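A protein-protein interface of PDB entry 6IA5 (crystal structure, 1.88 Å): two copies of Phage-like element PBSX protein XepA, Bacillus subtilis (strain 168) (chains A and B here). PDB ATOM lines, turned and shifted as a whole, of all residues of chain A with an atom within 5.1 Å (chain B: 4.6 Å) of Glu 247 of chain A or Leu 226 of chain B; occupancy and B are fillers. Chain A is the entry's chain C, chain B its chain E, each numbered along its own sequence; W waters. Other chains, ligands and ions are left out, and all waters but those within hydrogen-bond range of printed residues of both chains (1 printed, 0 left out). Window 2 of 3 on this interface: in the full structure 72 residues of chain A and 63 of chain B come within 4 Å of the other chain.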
ATOM      1  N   VAL A 203      -7.229   2.870  29.314  1.00  0.00           N
ATOM      2  CA  VAL A 203      -6.348   2.412  30.376  1.00  0.00           C
ATOM      3  C   VAL A 203      -6.285   0.885  30.349  1.00  0.00           C
ATOM      4  O   VAL A 203      -7.318   0.233  30.408  1.00  0.00           O
ATOM      5  CB  VAL A 203      -6.825   2.885  31.769  1.00  0.00           C
ATOM      6  CG1 VAL A 203      -5.940   2.309  32.874  1.00  0.00           C
ATOM      7  CG2 VAL A 203      -6.893   4.408  31.886  1.00  0.00           C
ATOM      8  N   GLU A 204      -5.065   0.344  30.313  1.00  0.00           N
ATOM      9  CA  GLU A 204      -4.827  -1.085  30.445  1.00  0.00           C
ATOM     10  C   GLU A 204      -4.330  -1.411  31.856  1.00  0.00           C
ATOM     11  O   GLU A 204      -3.440  -0.745  32.372  1.00  0.00           O
ATOM     12  CB  GLU A 204      -3.830  -1.579  29.397  1.00  0.00           C
ATOM     13  CG  GLU A 204      -3.883  -3.093  29.224  1.00  0.00           C
ATOM     14  CD  GLU A 204      -2.828  -3.724  28.306  1.00  0.00           C
ATOM     15  OE1 GLU A 204      -2.568  -4.951  28.439  1.00  0.00           O
ATOM     16  OE2 GLU A 204      -2.258  -3.013  27.445  1.00  0.00           O
ATOM     17  N   VAL A 205      -4.906  -2.458  32.456  1.00  0.00           N
ATOM     18  CA  VAL A 205      -4.514  -3.002  33.744  1.00  0.00           C
ATOM     19  C   VAL A 205      -3.986  -4.419  33.503  1.00  0.00           C
ATOM     20  O   VAL A 205      -4.687  -5.253  32.930  1.00  0.00           O
ATOM     21  CB  VAL A 205      -5.707  -3.005  34.726  1.00  0.00           C
ATOM     22  CG1 VAL A 205      -5.350  -3.599  36.078  1.00  0.00           C
ATOM     23  CG2 VAL A 205      -6.303  -1.611  34.917  1.00  0.00           C
ATOM     24  N   LYS A 232     -15.454  -1.042  29.984  1.00  0.00           N
ATOM     25  CA  LYS A 232     -14.531  -2.126  29.671  1.00  0.00           C
ATOM     26  C   LYS A 232     -14.691  -2.532  28.209  1.00  0.00           C
ATOM     27  O   LYS A 232     -15.812  -2.621  27.717  1.00  0.00           O
ATOM     28  CB  LYS A 232     -14.767  -3.291  30.627  1.00  0.00           C
ATOM     29  CG  LYS A 232     -13.765  -4.440  30.486  1.00  0.00           C
ATOM     30  CD  LYS A 232     -13.466  -5.144  31.798  1.00  0.00           C
ATOM     31  CE  LYS A 232     -14.618  -6.027  32.244  1.00  0.00           C
ATOM     32  NZ  LYS A 232     -14.750  -7.218  31.364  1.00  0.00           N
ATOM     33  N   THR A 233     -13.572  -2.756  27.495  1.00  0.00           N
ATOM     34  CA  THR A 233     -13.656  -2.916  26.045  1.00  0.00           C
ATOM     35  C   THR A 233     -14.359  -4.231  25.663  1.00  0.00           C
ATOM     36  O   THR A 233     -15.035  -4.282  24.645  1.00  0.00           O
ATOM     37  CB  THR A 233     -12.293  -2.808  25.345  1.00  0.00           C
ATOM     38  OG1 THR A 233     -11.500  -3.934  25.751  1.00  0.00           O
ATOM     39  CG2 THR A 233     -11.578  -1.502  25.628  1.00  0.00           C
ATOM     40  N   THR A 242     -12.245  -1.628  39.406  1.00  0.00           N
ATOM     41  CA  THR A 242     -12.146  -2.995  38.920  1.00  0.00           C
ATOM     42  C   THR A 242     -11.326  -3.852  39.881  1.00  0.00           C
ATOM     43  O   THR A 242     -10.372  -3.368  40.492  1.00  0.00           O
ATOM     44  CB  THR A 242     -11.583  -3.052  37.494  1.00  0.00           C
ATOM     45  OG1 THR A 242     -11.650  -4.412  37.080  1.00  0.00           O
ATOM     46  CG2 THR A 242     -10.145  -2.597  37.373  1.00  0.00           C
ATOM     47  N   GLY A 244     -10.316  -6.682  38.370  1.00  0.00           N
ATOM     48  CA  GLY A 244      -9.793  -7.519  37.297  1.00  0.00           C
ATOM     49  C   GLY A 244      -8.462  -6.998  36.758  1.00  0.00           C
ATOM     50  O   GLY A 244      -7.980  -5.947  37.167  1.00  0.00           O
ATOM     51  N   LYS A 245      -7.880  -7.743  35.816  1.00  0.00           N
ATOM     52  CA  LYS A 245      -6.666  -7.354  35.116  1.00  0.00           C
ATOM     53  C   LYS A 245      -6.692  -8.026  33.747  1.00  0.00           C
ATOM     54  O   LYS A 245      -7.628  -8.761  33.459  1.00  0.00           O
ATOM     55  CB  LYS A 245      -5.447  -7.795  35.921  1.00  0.00           C
ATOM     56  CG  LYS A 245      -5.292  -9.300  36.030  1.00  0.00           C
ATOM     57  CD  LYS A 245      -4.067  -9.723  36.803  1.00  0.00           C
ATOM     58  CE  LYS A 245      -4.042 -11.221  36.980  1.00  0.00           C
ATOM     59  NZ  LYS A 245      -2.681 -11.674  37.335  1.00  0.00           N
ATOM     60  N   ALA A 246      -5.670  -7.786  32.919  1.00  0.00           N
ATOM     61  CA  ALA A 246      -5.722  -8.159  31.513  1.00  0.00           C
ATOM     62  C   ALA A 246      -7.006  -7.586  30.900  1.00  0.00           C
ATOM     63  O   ALA A 246      -7.769  -8.280  30.230  1.00  0.00           O
ATOM     64  CB  ALA A 246      -5.621  -9.668  31.341  1.00  0.00           C
ATOM     65  N   GLU A 247      -7.246  -6.299  31.166  1.00  0.00           N
ATOM     66  CA  GLU A 247      -8.443  -5.643  30.677  1.00  0.00           C
ATOM     67  C   GLU A 247      -8.131  -4.173  30.421  1.00  0.00           C
ATOM     68  O   GLU A 247      -7.107  -3.665  30.884  1.00  0.00           O
ATOM     69  CB  GLU A 247      -9.623  -5.848  31.642  1.00  0.00           C
ATOM     70  CG  GLU A 247      -9.339  -5.361  33.038  1.00  0.00           C
ATOM     71  CD  GLU A 247     -10.444  -5.599  34.056  1.00  0.00           C
ATOM     72  OE1 GLU A 247     -10.573  -4.757  34.979  1.00  0.00           O
ATOM     73  OE2 GLU A 247     -11.170  -6.633  33.948  1.00  0.00           O
ATOM     74  N   ALA A 248      -9.001  -3.529  29.639  1.00  0.00           N
ATOM     75  CA  ALA A 248      -8.809  -2.144  29.251  1.00  0.00           C
ATOM     76  C   ALA A 248     -10.133  -1.409  29.434  1.00  0.00           C
ATOM     77  O   ALA A 248     -11.196  -1.949  29.117  1.00  0.00           O
ATOM     78  CB  ALA A 248      -8.304  -2.042  27.826  1.00  0.00           C
ATOM     79  N   TRP A 249     -10.035  -0.163  29.917  1.00  0.00           N
ATOM     80  CA  TRP A 249     -11.174   0.655  30.284  1.00  0.00           C
ATOM     81  C   TRP A 249     -11.079   1.973  29.531  1.00  0.00           C
ATOM     82  O   TRP A 249     -10.023   2.606  29.538  1.00  0.00           O
ATOM     83  CB  TRP A 249     -11.152   0.880  31.796  1.00  0.00           C
ATOM     84  CG  TRP A 249     -11.442  -0.359  32.592  1.00  0.00           C
ATOM     85  CD1 TRP A 249     -10.548  -1.313  32.991  1.00  0.00           C
ATOM     86  CD2 TRP A 249     -12.729  -0.781  33.088  1.00  0.00           C
ATOM     87  NE1 TRP A 249     -11.184  -2.293  33.704  1.00  0.00           N
ATOM     88  CE2 TRP A 249     -12.522  -2.001  33.778  1.00  0.00           C
ATOM     89  CE3 TRP A 249     -14.027  -0.251  33.021  1.00  0.00           C
ATOM     90  CZ2 TRP A 249     -13.571  -2.688  34.399  1.00  0.00           C
ATOM     91  CZ3 TRP A 249     -15.060  -0.932  33.633  1.00  0.00           C
ATOM     92  CH2 TRP A 249     -14.834  -2.132  34.308  1.00  0.00           C
ATOM     93  N   PHE B 216     -12.042 -10.298  17.564  1.00  0.00           N
ATOM     94  CA  PHE B 216     -11.654  -8.899  17.434  1.00  0.00           C
ATOM     95  C   PHE B 216     -10.735  -8.508  18.591  1.00  0.00           C
ATOM     96  O   PHE B 216     -11.096  -8.675  19.757  1.00  0.00           O
ATOM     97  CB  PHE B 216     -12.899  -8.005  17.446  1.00  0.00           C
ATOM     98  CG  PHE B 216     -14.030  -8.431  16.535  1.00  0.00           C
ATOM     99  CD1 PHE B 216     -13.781  -9.046  15.311  1.00  0.00           C
ATOM    100  CD2 PHE B 216     -15.355  -8.181  16.887  1.00  0.00           C
ATOM    101  CE1 PHE B 216     -14.829  -9.400  14.463  1.00  0.00           C
ATOM    102  CE2 PHE B 216     -16.398  -8.538  16.041  1.00  0.00           C
ATOM    103  CZ  PHE B 216     -16.128  -9.144  14.831  1.00  0.00           C
ATOM    104  N   TRP B 217      -9.552  -7.978  18.259  1.00  0.00           N
ATOM    105  CA  TRP B 217      -8.556  -7.665  19.274  1.00  0.00           C
ATOM    106  C   TRP B 217      -8.026  -6.255  19.062  1.00  0.00           C
ATOM    107  O   TRP B 217      -7.868  -5.817  17.930  1.00  0.00           O
ATOM    108  CB  TRP B 217      -7.354  -8.609  19.177  1.00  0.00           C
ATOM    109  CG  TRP B 217      -7.564 -10.073  19.407  1.00  0.00           C
ATOM    110  CD1 TRP B 217      -7.514 -11.053  18.458  1.00  0.00           C
ATOM    111  CD2 TRP B 217      -7.724 -10.748  20.668  1.00  0.00           C
ATOM    112  NE1 TRP B 217      -7.652 -12.287  19.038  1.00  0.00           N
ATOM    113  CE2 TRP B 217      -7.771 -12.137  20.393  1.00  0.00           C
ATOM    114  CE3 TRP B 217      -7.824 -10.327  22.000  1.00  0.00           C
ATOM    115  CZ2 TRP B 217      -7.932 -13.097  21.395  1.00  0.00           C
ATOM    116  CZ3 TRP B 217      -7.983 -11.274  22.994  1.00  0.00           C
ATOM    117  CH2 TRP B 217      -8.042 -12.640  22.692  1.00  0.00           C
ATOM    118  N   GLY B 218      -7.699  -5.589  20.173  1.00  0.00           N
ATOM    119  CA  GLY B 218      -6.862  -4.404  20.151  1.00  0.00           C
ATOM    120  C   GLY B 218      -5.596  -4.644  20.975  1.00  0.00           C
ATOM    121  O   GLY B 218      -5.567  -5.531  21.828  1.00  0.00           O
ATOM    122  N   SER B 220      -2.976  -2.274  23.377  1.00  0.00           N
ATOM    123  CA  SER B 220      -2.668  -0.998  24.005  1.00  0.00           C
ATOM    124  C   SER B 220      -1.183  -1.000  24.379  1.00  0.00           C
ATOM    125  O   SER B 220      -0.361  -1.521  23.638  1.00  0.00           O
ATOM    126  CB  SER B 220      -3.573  -0.765  25.195  1.00  0.00           C
ATOM    127  OG  SER B 220      -3.386   0.533  25.750  1.00  0.00           O
ATOM    128  N   GLN B 224      -0.145  -6.871  24.969  1.00  0.00           N
ATOM    129  CA  GLN B 224      -1.072  -7.991  25.057  1.00  0.00           C
ATOM    130  C   GLN B 224      -2.358  -7.671  24.287  1.00  0.00           C
ATOM    131  O   GLN B 224      -2.836  -6.541  24.290  1.00  0.00           O
ATOM    132  CB  GLN B 224      -1.419  -8.297  26.510  1.00  0.00           C
ATOM    133  CG  GLN B 224      -0.221  -8.796  27.322  1.00  0.00           C
ATOM    134  CD  GLN B 224       0.315 -10.107  26.795  1.00  0.00           C
ATOM    135  OE1 GLN B 224      -0.379 -11.118  26.789  1.00  0.00           O
ATOM    136  NE2 GLN B 224       1.551 -10.100  26.323  1.00  0.00           N
ATOM    137  N   LYS B 225      -2.918  -8.697  23.641  1.00  0.00           N
ATOM    138  CA  LYS B 225      -4.181  -8.597  22.936  1.00  0.00           C
ATOM    139  C   LYS B 225      -5.310  -8.441  23.950  1.00  0.00           C
ATOM    140  O   LYS B 225      -5.363  -9.154  24.954  1.00  0.00           O
ATOM    141  CB  LYS B 225      -4.397  -9.819  22.034  1.00  0.00           C
ATOM    142  CG  LYS B 225      -3.478  -9.864  20.818  1.00  0.00           C
ATOM    143  CD  LYS B 225      -3.930 -10.831  19.746  1.00  0.00           C
ATOM    144  CE  LYS B 225      -4.171 -12.252  20.220  1.00  0.00           C
ATOM    145  NZ  LYS B 225      -2.943 -12.849  20.773  1.00  0.00           N
ATOM    146  N   LEU B 226      -6.197  -7.478  23.667  1.00  0.00           N
ATOM    147  CA  LEU B 226      -7.369  -7.180  24.476  1.00  0.00           C
ATOM    148  C   LEU B 226      -8.605  -7.325  23.592  1.00  0.00           C
ATOM    149  O   LEU B 226      -8.624  -6.808  22.471  1.00  0.00           O
ATOM    150  CB  LEU B 226      -7.262  -5.734  24.973  1.00  0.00           C
ATOM    151  CG  LEU B 226      -6.085  -5.466  25.908  1.00  0.00           C
ATOM    152  CD1 LEU B 226      -5.590  -4.030  25.764  1.00  0.00           C
ATOM    153  CD2 LEU B 226      -6.484  -5.768  27.345  1.00  0.00           C
ATOM    154  N   PRO B 227      -9.670  -7.997  24.074  1.00  0.00           N
ATOM    155  CA  PRO B 227     -10.882  -8.167  23.271  1.00  0.00           C
ATOM    156  C   PRO B 227     -11.575  -6.817  23.114  1.00  0.00           C
ATOM    157  O   PRO B 227     -11.659  -6.045  24.061  1.00  0.00           O
ATOM    158  CB  PRO B 227     -11.763  -9.129  24.084  1.00  0.00           C
ATOM    159  CG  PRO B 227     -10.879  -9.619  25.230  1.00  0.00           C
ATOM    160  CD  PRO B 227      -9.778  -8.595  25.413  1.00  0.00           C
ATOM    161  N   ILE B 228     -12.065  -6.546  21.902  1.00  0.00           N
ATOM    162  CA  ILE B 228     -12.845  -5.342  21.626  1.00  0.00           C
ATOM    163  C   ILE B 228     -14.171  -5.750  20.991  1.00  0.00           C
ATOM    164  O   ILE B 228     -14.298  -6.859  20.472  1.00  0.00           O
ATOM    165  CB  ILE B 228     -12.044  -4.376  20.729  1.00  0.00           C
ATOM    166  CG1 ILE B 228     -11.717  -5.019  19.375  1.00  0.00           C
ATOM    167  CG2 ILE B 228     -10.772  -3.961  21.463  1.00  0.00           C
ATOM    168  CD1 ILE B 228     -11.079  -4.101  18.380  1.00  0.00           C
ATOM    169  N   PHE B 256      -6.319   2.840  21.065  1.00  0.00           N
ATOM    170  CA  PHE B 256      -5.568   1.612  20.823  1.00  0.00           C
ATOM    171  C   PHE B 256      -4.330   1.909  19.978  1.00  0.00           C
ATOM    172  O   PHE B 256      -4.319   2.872  19.222  1.00  0.00           O
ATOM    173  CB  PHE B 256      -6.436   0.549  20.130  1.00  0.00           C
ATOM    174  CG  PHE B 256      -7.408  -0.137  21.051  1.00  0.00           C
ATOM    175  CD1 PHE B 256      -6.987  -1.152  21.901  1.00  0.00           C
ATOM    176  CD2 PHE B 256      -8.734   0.269  21.107  1.00  0.00           C
ATOM    177  CE1 PHE B 256      -7.879  -1.771  22.764  1.00  0.00           C
ATOM    178  CE2 PHE B 256      -9.613  -0.327  22.002  1.00  0.00           C
ATOM    179  CZ  PHE B 256      -9.193  -1.359  22.815  1.00  0.00           C
HETATM  180  O   HOH W   1      -2.023  -4.172  24.951  1.00  0.00           O
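Among the printed residues, merely in contact across the chains: Glu 204 of chain A with Ser 220 of chain B (3.4 Å), Thr 233 of chain A with Phe 256 of chain B (3.7 Å), Glu 204 of chain A with Leu 226 of chain B (3.8 Å), Glu 247 of chain A with Leu 226 of chain B (3.8 Å), Thr 233 of chain A with Ile 228 of chain B (3.9 Å) and Ala 248 of chain A with Leu 226 of chain B (3.9 Å).
O of Glu 247 of chain A lies within hydrogen-bond range of N of Val 205 of chain A, 3.0 Å away. N of Thr 233 of chain A is in hydrogen-bond range of O of Ala 248 of chain A, 3.0 Å away. OE1 of Glu 247 of chain A lies within hydrogen-bond range of NE1 of Trp 249 of chain A (2.8 Å). O of Phe 216 of chain B sits at hydrogen-bond distance from N of Ile 228 of chain B, 3.2 Å away. O of Gly 218 of chain B sits at hydrogen-bond distance from N of Leu 226 of chain B (2.8 Å).
No position is printed for both chains. Of the 7 pairs that touch across the chains among the printed residues, none has its exchanged pair printed and touching as well.
Water W1 lies within hydrogen-bond range of O of Gln 224 of chain B (2.6 Å), N of Ser 220 of chain B (2.6 Å) and OE2 of Glu 204 of chain A (2.8 Å).
Of chain B, only Leu 226 (3.8 Å) comes within 4 Å of Glu 247 of chain A. Of chain A, only Glu 204 (3.8 Å), Glu 247 (3.8 Å) and Ala 248 (3.9 Å) come within 4 Å of Leu 226 of chain B. Of the printed residues of chain A, Phe 256 of chain B touches Thr 233 (3.7 Å). Of the printed residues of chain B, Thr 233 of chain A touches Pro 227, Ile 228 and Phe 256. Of the printed residues of chain A, Ser 220 of chain B touches Glu 204. Of the printed residues of chain B, Ala 248 of chain A touches Leu 226 (3.9 Å). Of the printed residues of chain B, Glu 204 of chain A touches Ser 220 and Leu 226. The nearest residue of chain A that does not touch Leu 226 of chain B is Ala 246 of chain A (4.03 Å). The nearest printed residue of chain B that does not touch Thr 233 of chain A is Leu 226 of chain B (4.7 Å).
The side-chain hydroxyl (OG1) of Thr 233 of chain A is in hydrogen-bond range of the backbone carbonyl oxygen (O) of Pro 227 of chain B.
Of the 12 printed residues of chain A, 4 touch a printed residue of chain B. Among the printed residues, 7 pairs touch across the chains.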
